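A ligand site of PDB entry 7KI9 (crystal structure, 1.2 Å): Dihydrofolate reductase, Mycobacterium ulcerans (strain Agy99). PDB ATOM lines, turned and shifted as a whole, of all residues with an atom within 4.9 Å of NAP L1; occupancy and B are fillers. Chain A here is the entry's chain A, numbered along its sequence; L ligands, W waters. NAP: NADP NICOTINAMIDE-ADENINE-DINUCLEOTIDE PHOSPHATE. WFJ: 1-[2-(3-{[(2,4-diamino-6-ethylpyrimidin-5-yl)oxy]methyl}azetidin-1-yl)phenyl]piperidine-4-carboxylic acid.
The side-chain hydroxyl (OG1) of Thr 76 lies within hydrogen-bond range of the backbone NH (N) of Gln 78, 2.9 Å away.
The backbone carbonyl oxygen (O) of Thr 56 lies within hydrogen-bond range of the side-chain hydroxyl (OG) of Ser 59.
N of Arg 54 sits at hydrogen-bond distance from O of Val 75 (3.2 Å).
N of Ile 24 is in hydrogen-bond range of O of Ala 140 (2.8 Å).
O of Gly 25 sits at hydrogen-bond distance from N of Ala 140 (2.9 Å).
N of Gly 53 lies within hydrogen-bond range of O of Gly 109 (2.8 Å).
OH of Tyr 114 sits close to N of Gly 109, at 3.4 Å.
OH of Tyr 114 lies within hydrogen-bond range of O of Ile 15.
The backbone carbonyl oxygen (O) of Val 75 lies close to an oxygen (O4B) of NAP L1.
Residues that only touch NAP L1: Trp 16 (3.4 Å), Gly 25 (3.4 Å), Arg 26 (3.7 Å), Gly 28 (3.7 Å), Ile 30 (3.7 Å), Gly 53 (3.5 Å), Gly 90 (3.4 Å), Ile 108 (3.1 Å), Gly 109 (3.7 Å), Tyr 114 (3.6 Å) and Leu 116 (3.6 Å).
Hydrophobic or aromatic side chains within 4 Å of NAP L1: Trp 16, Ile 24, Ile 30, Val 75, Ala 111, Ile 113 and Leu 116.
The nearest printed residue that does not touch NAP L1 is Ser 59 (4.1 Å).
Water W4 lies within hydrogen-bond range of NH1 of Arg 77 and O1X of NAP L1.
Water W1 lies within hydrogen-bond range of an oxygen (O2D) of NAP L1 (2.7 Å) and the side-chain hydroxyl (OG) of Ser 59 (2.8 Å).
Water W8 lies within hydrogen-bond range of an oxygen (O2X) of NAP L1 and the guanidinium group (NH2) of Arg 54.
Water W6 lies within hydrogen-bond range of a nitrogen (N1A) of NAP L1 (2.8 Å) and the backbone carbonyl oxygen of Gly 90 (2.9 Å).
Water W2 bridges O1N of NAP L1 and NE2 of Gln 112.
The side-chain hydroxyl (OG1) of Thr 76 is in hydrogen-bond range of an oxygen (O3X) of NAP L1 (2.6 Å).
N of Thr 56 sits at hydrogen-bond distance from O1A of NAP L1.
The side-chain hydroxyl (OG1) of Thr 56 sits at hydrogen-bond distance from an oxygen (O1A) of NAP L1 (2.7 Å).
An oxygen (O5B) of NAP L1 is in hydrogen-bond range of the backbone NH (N) of Arg 55, at 3.3 Å.
The guanidinium group of Arg 55 is in hydrogen-bond range of an oxygen (O3B) of NAP L1, 2.8 Å away.
An oxygen (O7N) of NAP L1 lies within hydrogen-bond range of the backbone NH of Ala 17 (2.9 Å).
A nitrogen (N7N) of NAP L1 is in hydrogen-bond range of the backbone carbonyl oxygen of Ala 17 (2.8 Å).
N of Arg 54 sits at hydrogen-bond distance from O4B of NAP L1 (3.4 Å).
NE of Arg 54 lies within salt-bridge range of O3X of NAP L1 (2.8 Å).
An oxygen (O1X) of NAP L1 is in hydrogen-bond range of the backbone NH of Arg 77 (2.8 Å).
The guanidinium group (NH2) of Arg 77 lies close to a nitrogen (N7A) of NAP L1, 3.5 Å away.
N of Gln 112 is in hydrogen-bond range of O1N of NAP L1 (2.9 Å).
NE2 of Gln 78 lies within hydrogen-bond range of O3X of NAP L1 (2.9 Å).
N of Gly 110 sits at hydrogen-bond distance from O1A of NAP L1 (3.0 Å).
O of Ile 24 sits at hydrogen-bond distance from N7N of NAP L1 (3.0 Å).
N of Ala 111 sits at hydrogen-bond distance from O1N of NAP L1 (3.0 Å).
The backbone NH (N) of Gly 29 sits at hydrogen-bond distance from an oxygen (O3D) of NAP L1 (3.5 Å).
O of Gly 29 lies within hydrogen-bond range of O3D of NAP L1 (3.1 Å).
The backbone NH (N) of Ile 113 sits at hydrogen-bond distance from an oxygen (O2A) of NAP L1, 3.1 Å away.
The backbone carbonyl oxygen (O) of Ile 108 is in hydrogen-bond range of a nitrogen (N09) of WFJ L2, at 3.0 Å.
The side-chain hydroxyl of Tyr 114 lies within hydrogen-bond range of a nitrogen (N09) of WFJ L2 (3.5 Å).
O of Ile 15 lies within hydrogen-bond range of N09 of WFJ L2 (2.8 Å).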
ATOM      1  N   ILE A  15       9.628 -15.813  34.408  1.00  0.00           N
ATOM      2  CA  ILE A  15       8.832 -15.961  35.615  1.00  0.00           C
ATOM      3  C   ILE A  15       7.383 -15.670  35.256  1.00  0.00           C
ATOM      4  O   ILE A  15       7.098 -14.651  34.607  1.00  0.00           O
ATOM      5  CB  ILE A  15       9.356 -15.080  36.775  1.00  0.00           C
ATOM      6  CG1 ILE A  15       8.548 -15.315  38.058  1.00  0.00           C
ATOM      7  CG2 ILE A  15       9.437 -13.576  36.404  1.00  0.00           C
ATOM      8  CD1 ILE A  15       9.219 -14.720  39.315  1.00  0.00           C
ATOM      9  N   TRP A  16       6.473 -16.570  35.630  1.00  0.00           N
ATOM     10  CA  TRP A  16       5.060 -16.379  35.333  1.00  0.00           C
ATOM     11  C   TRP A  16       4.228 -17.115  36.357  1.00  0.00           C
ATOM     12  O   TRP A  16       4.696 -18.040  37.028  1.00  0.00           O
ATOM     13  CB  TRP A  16       4.676 -16.830  33.911  1.00  0.00           C
ATOM     14  CG  TRP A  16       4.606 -18.317  33.640  1.00  0.00           C
ATOM     15  CD1 TRP A  16       3.522 -19.142  33.834  1.00  0.00           C
ATOM     16  CD2 TRP A  16       5.591 -19.140  32.991  1.00  0.00           C
ATOM     17  NE1 TRP A  16       3.791 -20.414  33.372  1.00  0.00           N
ATOM     18  CE2 TRP A  16       5.058 -20.438  32.861  1.00  0.00           C
ATOM     19  CE3 TRP A  16       6.888 -18.900  32.532  1.00  0.00           C
ATOM     20  CZ2 TRP A  16       5.775 -21.483  32.286  1.00  0.00           C
ATOM     21  CZ3 TRP A  16       7.590 -19.929  31.968  1.00  0.00           C
ATOM     22  CH2 TRP A  16       7.041 -21.212  31.849  1.00  0.00           C
ATOM     23  N   ALA A  17       2.953 -16.741  36.425  1.00  0.00           N
ATOM     24  CA  ALA A  17       1.937 -17.459  37.181  1.00  0.00           C
ATOM     25  C   ALA A  17       0.866 -17.953  36.218  1.00  0.00           C
ATOM     26  O   ALA A  17       0.489 -17.245  35.276  1.00  0.00           O
ATOM     27  CB  ALA A  17       1.318 -16.543  38.246  1.00  0.00           C
ATOM     28  N   ILE A  24      -2.565 -17.705  31.441  1.00  0.00           N
ATOM     29  CA  ILE A  24      -1.793 -16.642  32.091  1.00  0.00           C
ATOM     30  C   ILE A  24      -2.437 -15.275  31.953  1.00  0.00           C
ATOM     31  O   ILE A  24      -2.115 -14.390  32.750  1.00  0.00           O
ATOM     32  CB  ILE A  24      -0.319 -16.597  31.616  1.00  0.00           C
ATOM     33  CG1 ILE A  24      -0.184 -16.185  30.149  1.00  0.00           C
ATOM     34  CG2 ILE A  24       0.387 -17.910  31.918  1.00  0.00           C
ATOM     35  CD1 ILE A  24       1.240 -15.762  29.790  1.00  0.00           C
ATOM     36  N   GLY A  25      -3.329 -15.081  30.989  1.00  0.00           N
ATOM     37  CA  GLY A  25      -3.886 -13.753  30.782  1.00  0.00           C
ATOM     38  C   GLY A  25      -5.232 -13.829  30.117  1.00  0.00           C
ATOM     39  O   GLY A  25      -5.501 -14.742  29.322  1.00  0.00           O
ATOM     40  N   ARG A  26      -6.087 -12.861  30.429  1.00  0.00           N
ATOM     41  CA  ARG A  26      -7.427 -12.795  29.869  1.00  0.00           C
ATOM     42  C   ARG A  26      -7.896 -11.348  29.950  1.00  0.00           C
ATOM     43  O   ARG A  26      -7.723 -10.704  30.986  1.00  0.00           O
ATOM     44  CB  ARG A  26      -8.369 -13.708  30.648  1.00  0.00           C
ATOM     45  CG  ARG A  26      -9.832 -13.616  30.206  1.00  0.00           C
ATOM     46  CD  ARG A  26     -10.681 -14.599  30.965  1.00  0.00           C
ATOM     47  NE  ARG A  26     -10.312 -15.971  30.645  1.00  0.00           N
ATOM     48  CZ  ARG A  26     -10.789 -17.043  31.252  1.00  0.00           C
ATOM     49  NH1 ARG A  26     -11.663 -16.944  32.251  1.00  0.00           N
ATOM     50  NH2 ARG A  26     -10.402 -18.254  30.849  1.00  0.00           N
ATOM     51  N   GLY A  28      -6.771  -8.606  28.875  1.00  0.00           N
ATOM     52  CA  GLY A  28      -5.767  -7.615  29.183  1.00  0.00           C
ATOM     53  C   GLY A  28      -5.294  -7.615  30.608  1.00  0.00           C
ATOM     54  O   GLY A  28      -4.602  -6.678  31.018  1.00  0.00           O
ATOM     55  N   GLY A  29      -5.623  -8.637  31.376  1.00  0.00           N
ATOM     56  CA  GLY A  29      -5.159  -8.710  32.747  1.00  0.00           C
ATOM     57  C   GLY A  29      -4.913 -10.133  33.177  1.00  0.00           C
ATOM     58  O   GLY A  29      -4.863 -11.040  32.339  1.00  0.00           O
ATOM     59  N   ILE A  30      -4.779 -10.349  34.473  1.00  0.00           N
ATOM     60  CA  ILE A  30      -4.556 -11.666  35.030  1.00  0.00           C
ATOM     61  C   ILE A  30      -5.834 -12.079  35.745  1.00  0.00           C
ATOM     62  O   ILE A  30      -6.309 -11.341  36.630  1.00  0.00           O
ATOM     63  CB  ILE A  30      -3.330 -11.689  35.964  1.00  0.00           C
ATOM     64  CG1 ILE A  30      -2.041 -11.402  35.151  1.00  0.00           C
ATOM     65  CG2 ILE A  30      -3.256 -13.011  36.716  1.00  0.00           C
ATOM     66  CD1 ILE A  30      -0.791 -11.229  35.981  1.00  0.00           C
ATOM     67  N   TRP A  32      -7.012 -13.833  38.134  1.00  0.00           N
ATOM     68  CA  TRP A  32      -7.115 -14.228  39.540  1.00  0.00           C
ATOM     69  C   TRP A  32      -6.302 -13.214  40.332  1.00  0.00           C
ATOM     70  O   TRP A  32      -5.521 -12.456  39.763  1.00  0.00           O
ATOM     71  CB  TRP A  32      -6.582 -15.646  39.820  1.00  0.00           C
ATOM     72  CG  TRP A  32      -5.131 -15.764  39.469  1.00  0.00           C
ATOM     73  CD1 TRP A  32      -4.067 -15.372  40.207  1.00  0.00           C
ATOM     74  CD2 TRP A  32      -4.601 -16.233  38.216  1.00  0.00           C
ATOM     75  NE1 TRP A  32      -2.895 -15.573  39.516  1.00  0.00           N
ATOM     76  CE2 TRP A  32      -3.200 -16.102  38.284  1.00  0.00           C
ATOM     77  CE3 TRP A  32      -5.190 -16.730  37.052  1.00  0.00           C
ATOM     78  CZ2 TRP A  32      -2.378 -16.476  37.237  1.00  0.00           C
ATOM     79  CZ3 TRP A  32      -4.364 -17.109  36.018  1.00  0.00           C
ATOM     80  CH2 TRP A  32      -2.982 -16.966  36.113  1.00  0.00           C
ATOM     81  N   GLY A  53       6.819  -7.477  27.447  1.00  0.00           N
ATOM     82  CA  GLY A  53       6.179  -6.981  26.238  1.00  0.00           C
ATOM     83  C   GLY A  53       5.348  -5.751  26.508  1.00  0.00           C
ATOM     84  O   GLY A  53       4.894  -5.475  27.632  1.00  0.00           O
ATOM     85  N   ARG A  54       5.118  -4.986  25.429  1.00  0.00           N
ATOM     86  CA  ARG A  54       4.444  -3.718  25.592  1.00  0.00           C
ATOM     87  C   ARG A  54       3.004  -3.888  26.081  1.00  0.00           C
ATOM     88  O   ARG A  54       2.491  -3.040  26.813  1.00  0.00           O
ATOM     89  CB  ARG A  54       4.531  -2.914  24.293  1.00  0.00           C
ATOM     90  CG  ARG A  54       4.199  -1.409  24.400  1.00  0.00           C
ATOM     91  CD  ARG A  54       2.704  -1.086  24.292  1.00  0.00           C
ATOM     92  NE  ARG A  54       2.156  -1.714  23.105  1.00  0.00           N
ATOM     93  CZ  ARG A  54       0.923  -2.218  23.025  1.00  0.00           C
ATOM     94  NH1 ARG A  54       0.048  -2.060  24.005  1.00  0.00           N
ATOM     95  NH2 ARG A  54       0.575  -2.908  21.949  1.00  0.00           N
ATOM     96  N   ARG A  55       2.316  -4.959  25.692  1.00  0.00           N
ATOM     97  CA  ARG A  55       0.952  -5.124  26.179  1.00  0.00           C
ATOM     98  C   ARG A  55       0.935  -5.317  27.682  1.00  0.00           C
ATOM     99  O   ARG A  55       0.068  -4.752  28.377  1.00  0.00           O
ATOM    100  CB  ARG A  55       0.250  -6.265  25.428  1.00  0.00           C
ATOM    101  CG  ARG A  55       0.100  -5.928  23.951  1.00  0.00           C
ATOM    102  CD  ARG A  55      -0.690  -6.941  23.136  1.00  0.00           C
ATOM    103  NE  ARG A  55      -0.287  -6.857  21.731  1.00  0.00           N
ATOM    104  CZ  ARG A  55      -0.840  -7.527  20.730  1.00  0.00           C
ATOM    105  NH1 ARG A  55      -1.932  -8.262  20.903  1.00  0.00           N
ATOM    106  NH2 ARG A  55      -0.279  -7.461  19.531  1.00  0.00           N
ATOM    107  N   THR A  56       1.906  -6.060  28.227  1.00  0.00           N
ATOM    108  CA  THR A  56       2.011  -6.205  29.671  1.00  0.00           C
ATOM    109  C   THR A  56       2.291  -4.861  30.339  1.00  0.00           C
ATOM    110  O   THR A  56       1.682  -4.536  31.362  1.00  0.00           O
ATOM    111  CB  THR A  56       3.077  -7.258  30.006  1.00  0.00           C
ATOM    112  OG1 THR A  56       2.613  -8.539  29.563  1.00  0.00           O
ATOM    113  CG2 THR A  56       3.358  -7.334  31.489  1.00  0.00           C
ATOM    114  N   SER A  59      -0.816  -3.029  30.608  1.00  0.00           N
ATOM    115  CA  SER A  59      -1.754  -3.700  31.512  1.00  0.00           C
ATOM    116  C   SER A  59      -1.511  -3.386  32.975  1.00  0.00           C
ATOM    117  O   SER A  59      -2.378  -3.671  33.809  1.00  0.00           O
ATOM    118  CB  SER A  59      -1.692  -5.221  31.307  1.00  0.00           C
ATOM    119  OG  SER A  59      -0.598  -5.792  31.997  1.00  0.00           O
ATOM    120  N   VAL A  75       9.715  -4.246  25.455  1.00  0.00           N
ATOM    121  CA  VAL A  75       9.964  -4.653  24.081  1.00  0.00           C
ATOM    122  C   VAL A  75       8.766  -4.215  23.254  1.00  0.00           C
ATOM    123  O   VAL A  75       7.630  -4.627  23.520  1.00  0.00           O
ATOM    124  CB  VAL A  75      10.153  -6.178  24.002  1.00  0.00           C
ATOM    125  CG1 VAL A  75      10.437  -6.605  22.560  1.00  0.00           C
ATOM    126  CG2 VAL A  75      11.255  -6.632  24.970  1.00  0.00           C
ATOM    127  N   THR A  76       9.009  -3.395  22.228  1.00  0.00           N
ATOM    128  CA  THR A  76       7.964  -2.825  21.393  1.00  0.00           C
ATOM    129  C   THR A  76       8.543  -2.606  20.005  1.00  0.00           C
ATOM    130  O   THR A  76       9.746  -2.449  19.844  1.00  0.00           O
ATOM    131  CB  THR A  76       7.465  -1.492  21.992  1.00  0.00           C
ATOM    132  OG1 THR A  76       6.485  -0.889  21.145  1.00  0.00           O
ATOM    133  CG2 THR A  76       8.608  -0.511  22.191  1.00  0.00           C
ATOM    134  N   ARG A  77       7.650  -2.575  19.007  1.00  0.00           N
ATOM    135  CA  ARG A  77       8.051  -2.119  17.673  1.00  0.00           C
ATOM    136  C   ARG A  77       7.814  -0.630  17.486  1.00  0.00           C
ATOM    137  O   ARG A  77       8.190  -0.090  16.439  1.00  0.00           O
ATOM    138  CB  ARG A  77       7.301  -2.920  16.602  1.00  0.00           C
ATOM    139  CG  ARG A  77       7.651  -4.393  16.690  1.00  0.00           C
ATOM    140  CD  ARG A  77       6.865  -5.255  15.705  1.00  0.00           C
ATOM    141  NE  ARG A  77       7.097  -6.691  15.841  1.00  0.00           N
ATOM    142  CZ  ARG A  77       6.265  -7.561  16.396  1.00  0.00           C
ATOM    143  NH1 ARG A  77       5.161  -7.168  17.013  1.00  0.00           N
ATOM    144  NH2 ARG A  77       6.526  -8.864  16.324  1.00  0.00           N
ATOM    145  N   GLN A  78       7.217   0.052  18.459  1.00  0.00           N
ATOM    146  CA  GLN A  78       6.926   1.473  18.346  1.00  0.00           C
ATOM    147  C   GLN A  78       8.172   2.286  18.685  1.00  0.00           C
ATOM    148  O   GLN A  78       9.120   1.803  19.285  1.00  0.00           O
ATOM    149  CB  GLN A  78       5.814   1.852  19.318  1.00  0.00           C
ATOM    150  CG  GLN A  78       4.541   1.068  19.088  1.00  0.00           C
ATOM    151  CD  GLN A  78       3.411   1.572  19.953  1.00  0.00           C
ATOM    152  OE1 GLN A  78       2.987   2.718  19.805  1.00  0.00           O
ATOM    153  NE2 GLN A  78       2.934   0.732  20.865  1.00  0.00           N
ATOM    154  N   GLY A  90      13.747  -2.543  20.836  1.00  0.00           N
ATOM    155  CA  GLY A  90      13.034  -3.063  19.693  1.00  0.00           C
ATOM    156  C   GLY A  90      13.133  -4.547  19.488  1.00  0.00           C
ATOM    157  O   GLY A  90      12.600  -5.066  18.494  1.00  0.00           O
ATOM    158  N   SER A  91      13.813  -5.266  20.379  1.00  0.00           N
ATOM    159  CA  SER A  91      13.968  -6.708  20.247  1.00  0.00           C
ATOM    160  C   SER A  91      14.368  -7.265  21.601  1.00  0.00           C
ATOM    161  O   SER A  91      14.866  -6.539  22.476  1.00  0.00           O
ATOM    162  CB  SER A  91      15.033  -7.090  19.212  1.00  0.00           C
ATOM    163  OG  SER A  91      16.323  -6.722  19.684  1.00  0.00           O
ATOM    164  N   ILE A 108       9.218 -11.124  32.306  1.00  0.00           N
ATOM    165  CA  ILE A 108       8.047 -11.160  33.174  1.00  0.00           C
ATOM    166  C   ILE A 108       6.740 -11.186  32.402  1.00  0.00           C
ATOM    167  O   ILE A 108       5.681 -11.010  33.004  1.00  0.00           O
ATOM    168  CB  ILE A 108       8.063 -10.032  34.218  1.00  0.00           C
ATOM    169  CG1 ILE A 108       7.838  -8.664  33.561  1.00  0.00           C
ATOM    170  CG2 ILE A 108       9.406 -10.051  34.984  1.00  0.00           C
ATOM    171  CD1 ILE A 108       7.491  -7.571  34.575  1.00  0.00           C
ATOM    172  N   GLY A 109       6.795 -11.432  31.093  1.00  0.00           N
ATOM    173  CA  GLY A 109       5.593 -11.636  30.282  1.00  0.00           C
ATOM    174  C   GLY A 109       5.436 -10.569  29.214  1.00  0.00           C
ATOM    175  O   GLY A 109       6.231  -9.633  29.134  1.00  0.00           O
ATOM    176  N   GLY A 110       4.403 -10.715  28.378  1.00  0.00           N
ATOM    177  CA  GLY A 110       3.400 -11.762  28.408  1.00  0.00           C
ATOM    178  C   GLY A 110       3.745 -12.893  27.452  1.00  0.00           C
ATOM    179  O   GLY A 110       4.907 -13.219  27.252  1.00  0.00           O
ATOM    180  N   ALA A 111       2.703 -13.519  26.892  1.00  0.00           N
ATOM    181  CA  ALA A 111       2.904 -14.734  26.087  1.00  0.00           C
ATOM    182  C   ALA A 111       3.825 -14.490  24.892  1.00  0.00           C
ATOM    183  O   ALA A 111       4.652 -15.348  24.559  1.00  0.00           O
ATOM    184  CB  ALA A 111       1.558 -15.267  25.607  1.00  0.00           C
ATOM    185  N   GLN A 112       3.674 -13.359  24.218  1.00  0.00           N
ATOM    186  CA  GLN A 112       4.527 -13.121  23.047  1.00  0.00           C
ATOM    187  C   GLN A 112       5.987 -12.989  23.443  1.00  0.00           C
ATOM    188  O   GLN A 112       6.876 -13.568  22.806  1.00  0.00           O
ATOM    189  CB  GLN A 112       4.067 -11.885  22.277  1.00  0.00           C
ATOM    190  CG  GLN A 112       2.672 -11.992  21.739  1.00  0.00           C
ATOM    191  CD  GLN A 112       2.271 -10.801  20.916  1.00  0.00           C
ATOM    192  OE1 GLN A 112       3.129 -10.103  20.393  1.00  0.00           O
ATOM    193  NE2 GLN A 112       0.965 -10.570  20.793  1.00  0.00           N
ATOM    194  N   ILE A 113       6.244 -12.258  24.526  1.00  0.00           N
ATOM    195  CA  ILE A 113       7.622 -12.084  24.976  1.00  0.00           C
ATOM    196  C   ILE A 113       8.178 -13.376  25.595  1.00  0.00           C
ATOM    197  O   ILE A 113       9.364 -13.685  25.423  1.00  0.00           O
ATOM    198  CB  ILE A 113       7.729 -10.818  25.854  1.00  0.00           C
ATOM    199  CG1 ILE A 113       8.159  -9.619  25.016  1.00  0.00           C
ATOM    200  CG2 ILE A 113       8.710 -10.961  26.994  1.00  0.00           C
ATOM    201  CD1 ILE A 113       7.312  -9.308  23.809  1.00  0.00           C
ATOM    202  N   TYR A 114       7.334 -14.201  26.242  1.00  0.00           N
ATOM    203  CA  TYR A 114       7.823 -15.500  26.700  1.00  0.00           C
ATOM    204  C   TYR A 114       8.263 -16.352  25.524  1.00  0.00           C
ATOM    205  O   TYR A 114       9.274 -17.049  25.595  1.00  0.00           O
ATOM    206  CB  TYR A 114       6.770 -16.261  27.509  1.00  0.00           C
ATOM    207  CG  TYR A 114       6.438 -15.697  28.875  1.00  0.00           C
ATOM    208  CD1 TYR A 114       7.441 -15.258  29.740  1.00  0.00           C
ATOM    209  CD2 TYR A 114       5.125 -15.627  29.285  1.00  0.00           C
ATOM    210  CE1 TYR A 114       7.126 -14.745  31.002  1.00  0.00           C
ATOM    211  CE2 TYR A 114       4.800 -15.095  30.517  1.00  0.00           C
ATOM    212  CZ  TYR A 114       5.795 -14.665  31.366  1.00  0.00           C
ATOM    213  OH  TYR A 114       5.430 -14.125  32.576  1.00  0.00           O
ATOM    214  N   LEU A 116       9.459 -15.372  22.658  1.00  0.00           N
ATOM    215  CA  LEU A 116      10.752 -14.898  22.174  1.00  0.00           C
ATOM    216  C   LEU A 116      11.877 -15.311  23.108  1.00  0.00           C
ATOM    217  O   LEU A 116      12.999 -15.575  22.659  1.00  0.00           O
ATOM    218  CB  LEU A 116      10.752 -13.377  22.079  1.00  0.00           C
ATOM    219  CG  LEU A 116       9.872 -12.728  21.012  1.00  0.00           C
ATOM    220  CD1 LEU A 116       9.897 -11.205  21.163  1.00  0.00           C
ATOM    221  CD2 LEU A 116      10.337 -13.181  19.622  1.00  0.00           C
ATOM    222  N   ALA A 140      -4.346 -15.676  26.807  1.00  0.00           N
ATOM    223  CA  ALA A 140      -2.911 -15.932  26.723  1.00  0.00           C
ATOM    224  C   ALA A 140      -2.606 -17.158  27.560  1.00  0.00           C
ATOM    225  O   ALA A 140      -3.073 -17.262  28.711  1.00  0.00           O
ATOM    226  CB  ALA A 140      -2.138 -14.716  27.252  1.00  0.00           C
HETATM  227  PA  NAP L   1       2.992  -9.111  25.546  1.00  0.00           P
HETATM  228  O1A NAP L   1       3.008  -8.561  26.915  1.00  0.00           O
HETATM  229  O2A NAP L   1       3.927 -10.259  25.243  1.00  0.00           O
HETATM  230  O5B NAP L   1       3.277  -7.857  24.575  1.00  0.00           O
HETATM  231  C5B NAP L   1       3.142  -8.010  23.146  1.00  0.00           C
HETATM  232  C4B NAP L   1       3.778  -6.803  22.514  1.00  0.00           C
HETATM  233  O4B NAP L   1       5.214  -6.896  22.600  1.00  0.00           O
HETATM  234  C3B NAP L   1       3.479  -6.604  21.034  1.00  0.00           C
HETATM  235  O3B NAP L   1       2.198  -6.004  20.860  1.00  0.00           O
HETATM  236  C2B NAP L   1       4.641  -5.694  20.659  1.00  0.00           C
HETATM  237  O2B NAP L   1       4.517  -4.354  21.164  1.00  0.00           O
HETATM  238  C1B NAP L   1       5.787  -6.326  21.443  1.00  0.00           C
HETATM  239  N9A NAP L   1       6.490  -7.357  20.695  1.00  0.00           N
HETATM  240  C8A NAP L   1       6.144  -8.664  20.494  1.00  0.00           C
HETATM  241  N7A NAP L   1       6.964  -9.330  19.715  1.00  0.00           N
HETATM  242  C5A NAP L   1       7.937  -8.395  19.403  1.00  0.00           C
HETATM  243  C6A NAP L   1       9.111  -8.468  18.629  1.00  0.00           C
HETATM  244  N6A NAP L   1       9.522  -9.573  17.986  1.00  0.00           N
HETATM  245  N1A NAP L   1       9.857  -7.335  18.503  1.00  0.00           N
HETATM  246  C2A NAP L   1       9.448  -6.232  19.122  1.00  0.00           C
HETATM  247  N3A NAP L   1       8.365  -6.038  19.874  1.00  0.00           N
HETATM  248  C4A NAP L   1       7.655  -7.166  19.981  1.00  0.00           C
HETATM  249  O3  NAP L   1       1.505  -9.454  25.091  1.00  0.00           O
HETATM  250  PN  NAP L   1       0.559 -10.720  25.299  1.00  0.00           P
HETATM  251  O1N NAP L   1       1.230 -11.946  24.795  1.00  0.00           O
HETATM  252  O2N NAP L   1      -0.762 -10.345  24.748  1.00  0.00           O
HETATM  253  O5D NAP L   1       0.513 -10.875  26.881  1.00  0.00           O
HETATM  254  C5D NAP L   1      -0.274  -9.956  27.667  1.00  0.00           C
HETATM  255  C4D NAP L   1      -1.159 -10.763  28.582  1.00  0.00           C
HETATM  256  O4D NAP L   1      -0.348 -11.572  29.472  1.00  0.00           O
HETATM  257  C3D NAP L   1      -2.053  -9.931  29.503  1.00  0.00           C
HETATM  258  O3D NAP L   1      -3.268 -10.623  29.736  1.00  0.00           O
HETATM  259  C2D NAP L   1      -1.257  -9.887  30.801  1.00  0.00           C
HETATM  260  O2D NAP L   1      -2.090  -9.639  31.910  1.00  0.00           O
HETATM  261  C1D NAP L   1      -0.742 -11.322  30.803  1.00  0.00           C
HETATM  262  N1N NAP L   1       0.449 -11.522  31.703  1.00  0.00           N
HETATM  263  C2N NAP L   1       0.367 -12.531  32.593  1.00  0.00           C
HETATM  264  C3N NAP L   1       1.456 -12.818  33.403  1.00  0.00           C
HETATM  265  C7N NAP L   1       1.392 -13.942  34.396  1.00  0.00           C
HETATM  266  O7N NAP L   1       2.431 -14.286  34.965  1.00  0.00           O
HETATM  267  N7N NAP L   1       0.238 -14.558  34.572  1.00  0.00           N
HETATM  268  C4N NAP L   1       2.605 -12.034  33.274  1.00  0.00           C
HETATM  269  C5N NAP L   1       2.640 -10.994  32.364  1.00  0.00           C
HETATM  270  C6N NAP L   1       1.550 -10.755  31.569  1.00  0.00           C
HETATM  271  P2B NAP L   1       3.970  -3.197  20.207  1.00  0.00           P
HETATM  272  O1X NAP L   1       4.872  -3.163  18.999  1.00  0.00           O
HETATM  273  O2X NAP L   1       2.545  -3.600  19.867  1.00  0.00           O
HETATM  274  O3X NAP L   1       4.067  -1.971  21.074  1.00  0.00           O
HETATM  275  C01 WFJ L   2       2.163 -10.992  40.193  1.00  0.00           C
HETATM  276  C02 WFJ L   2       1.857 -11.555  38.783  1.00  0.00           C
HETATM  277  C03 WFJ L   2       3.049 -12.314  38.248  1.00  0.00           C
HETATM  278  C05 WFJ L   2       4.446 -14.110  38.521  1.00  0.00           C
HETATM  279  C08 WFJ L   2       4.829 -12.756  36.723  1.00  0.00           C
HETATM  280  C10 WFJ L   2       3.741 -11.953  37.124  1.00  0.00           C
HETATM  281  C12 WFJ L   2       4.098  -9.653  36.932  1.00  0.00           C
HETATM  282  C13 WFJ L   2       3.613  -8.384  36.279  1.00  0.00           C
HETATM  283  C14 WFJ L   2       2.087  -8.243  36.014  1.00  0.00           C
HETATM  284  C16 WFJ L   2       3.455  -7.211  37.308  1.00  0.00           C
HETATM  285  C17 WFJ L   2       0.880  -7.130  37.977  1.00  0.00           C
HETATM  286  C18 WFJ L   2      -0.372  -7.350  37.369  1.00  0.00           C
HETATM  287  C19 WFJ L   2      -1.557  -6.949  37.971  1.00  0.00           C
HETATM  288  C20 WFJ L   2      -1.532  -6.318  39.206  1.00  0.00           C
HETATM  289  C21 WFJ L   2      -0.298  -6.097  39.821  1.00  0.00           C
HETATM  290  C22 WFJ L   2       0.903  -6.490  39.232  1.00  0.00           C
HETATM  291  C24 WFJ L   2       2.566  -4.906  40.078  1.00  0.00           C
HETATM  292  C25 WFJ L   2       4.001  -4.749  40.619  1.00  0.00           C
HETATM  293  C26 WFJ L   2       4.275  -5.704  41.781  1.00  0.00           C
HETATM  294  C27 WFJ L   2       3.884  -7.139  41.398  1.00  0.00           C
HETATM  295  C28 WFJ L   2       2.425  -7.173  40.949  1.00  0.00           C
HETATM  296  C29 WFJ L   2       5.737  -5.706  42.088  1.00  0.00           C
HETATM  297  N04 WFJ L   2       3.416 -13.399  38.931  1.00  0.00           N
HETATM  298  N06 WFJ L   2       4.800 -15.174  39.272  1.00  0.00           N
HETATM  299  N07 WFJ L   2       5.177 -13.829  37.433  1.00  0.00           N
HETATM  300  N09 WFJ L   2       5.548 -12.488  35.611  1.00  0.00           N
HETATM  301  N15 WFJ L   2       2.021  -7.578  37.335  1.00  0.00           N
HETATM  302  N23 WFJ L   2       2.166  -6.290  39.844  1.00  0.00           N
HETATM  303  O11 WFJ L   2       3.410 -10.816  36.383  1.00  0.00           O
HETATM  304  O30 WFJ L   2       6.149  -4.617  42.807  1.00  0.00           O
HETATM  305  O31 WFJ L   2       6.513  -6.554  41.761  1.00  0.00           O
HETATM  306  O   HOH W   1      -1.020  -7.944  33.665  1.00  0.00           O
HETATM  307  O   HOH W   2      -0.368 -12.909  22.599  1.00  0.00           O
HETATM  308  O   HOH W   3       6.590 -11.696  18.634  1.00  0.00           O
HETATM  309  O   HOH W   4       3.988  -4.849  17.165  1.00  0.00           O
HETATM  310  O   HOH W   5       8.192 -11.971  16.598  1.00  0.00           O
HETATM  311  O   HOH W   6      11.941  -7.200  16.622  1.00  0.00           O
HETATM  312  O   HOH W   7       4.042  -1.646  16.924  1.00  0.00           O
HETATM  313  O   HOH W   8       0.786  -1.881  18.626  1.00  0.00           O
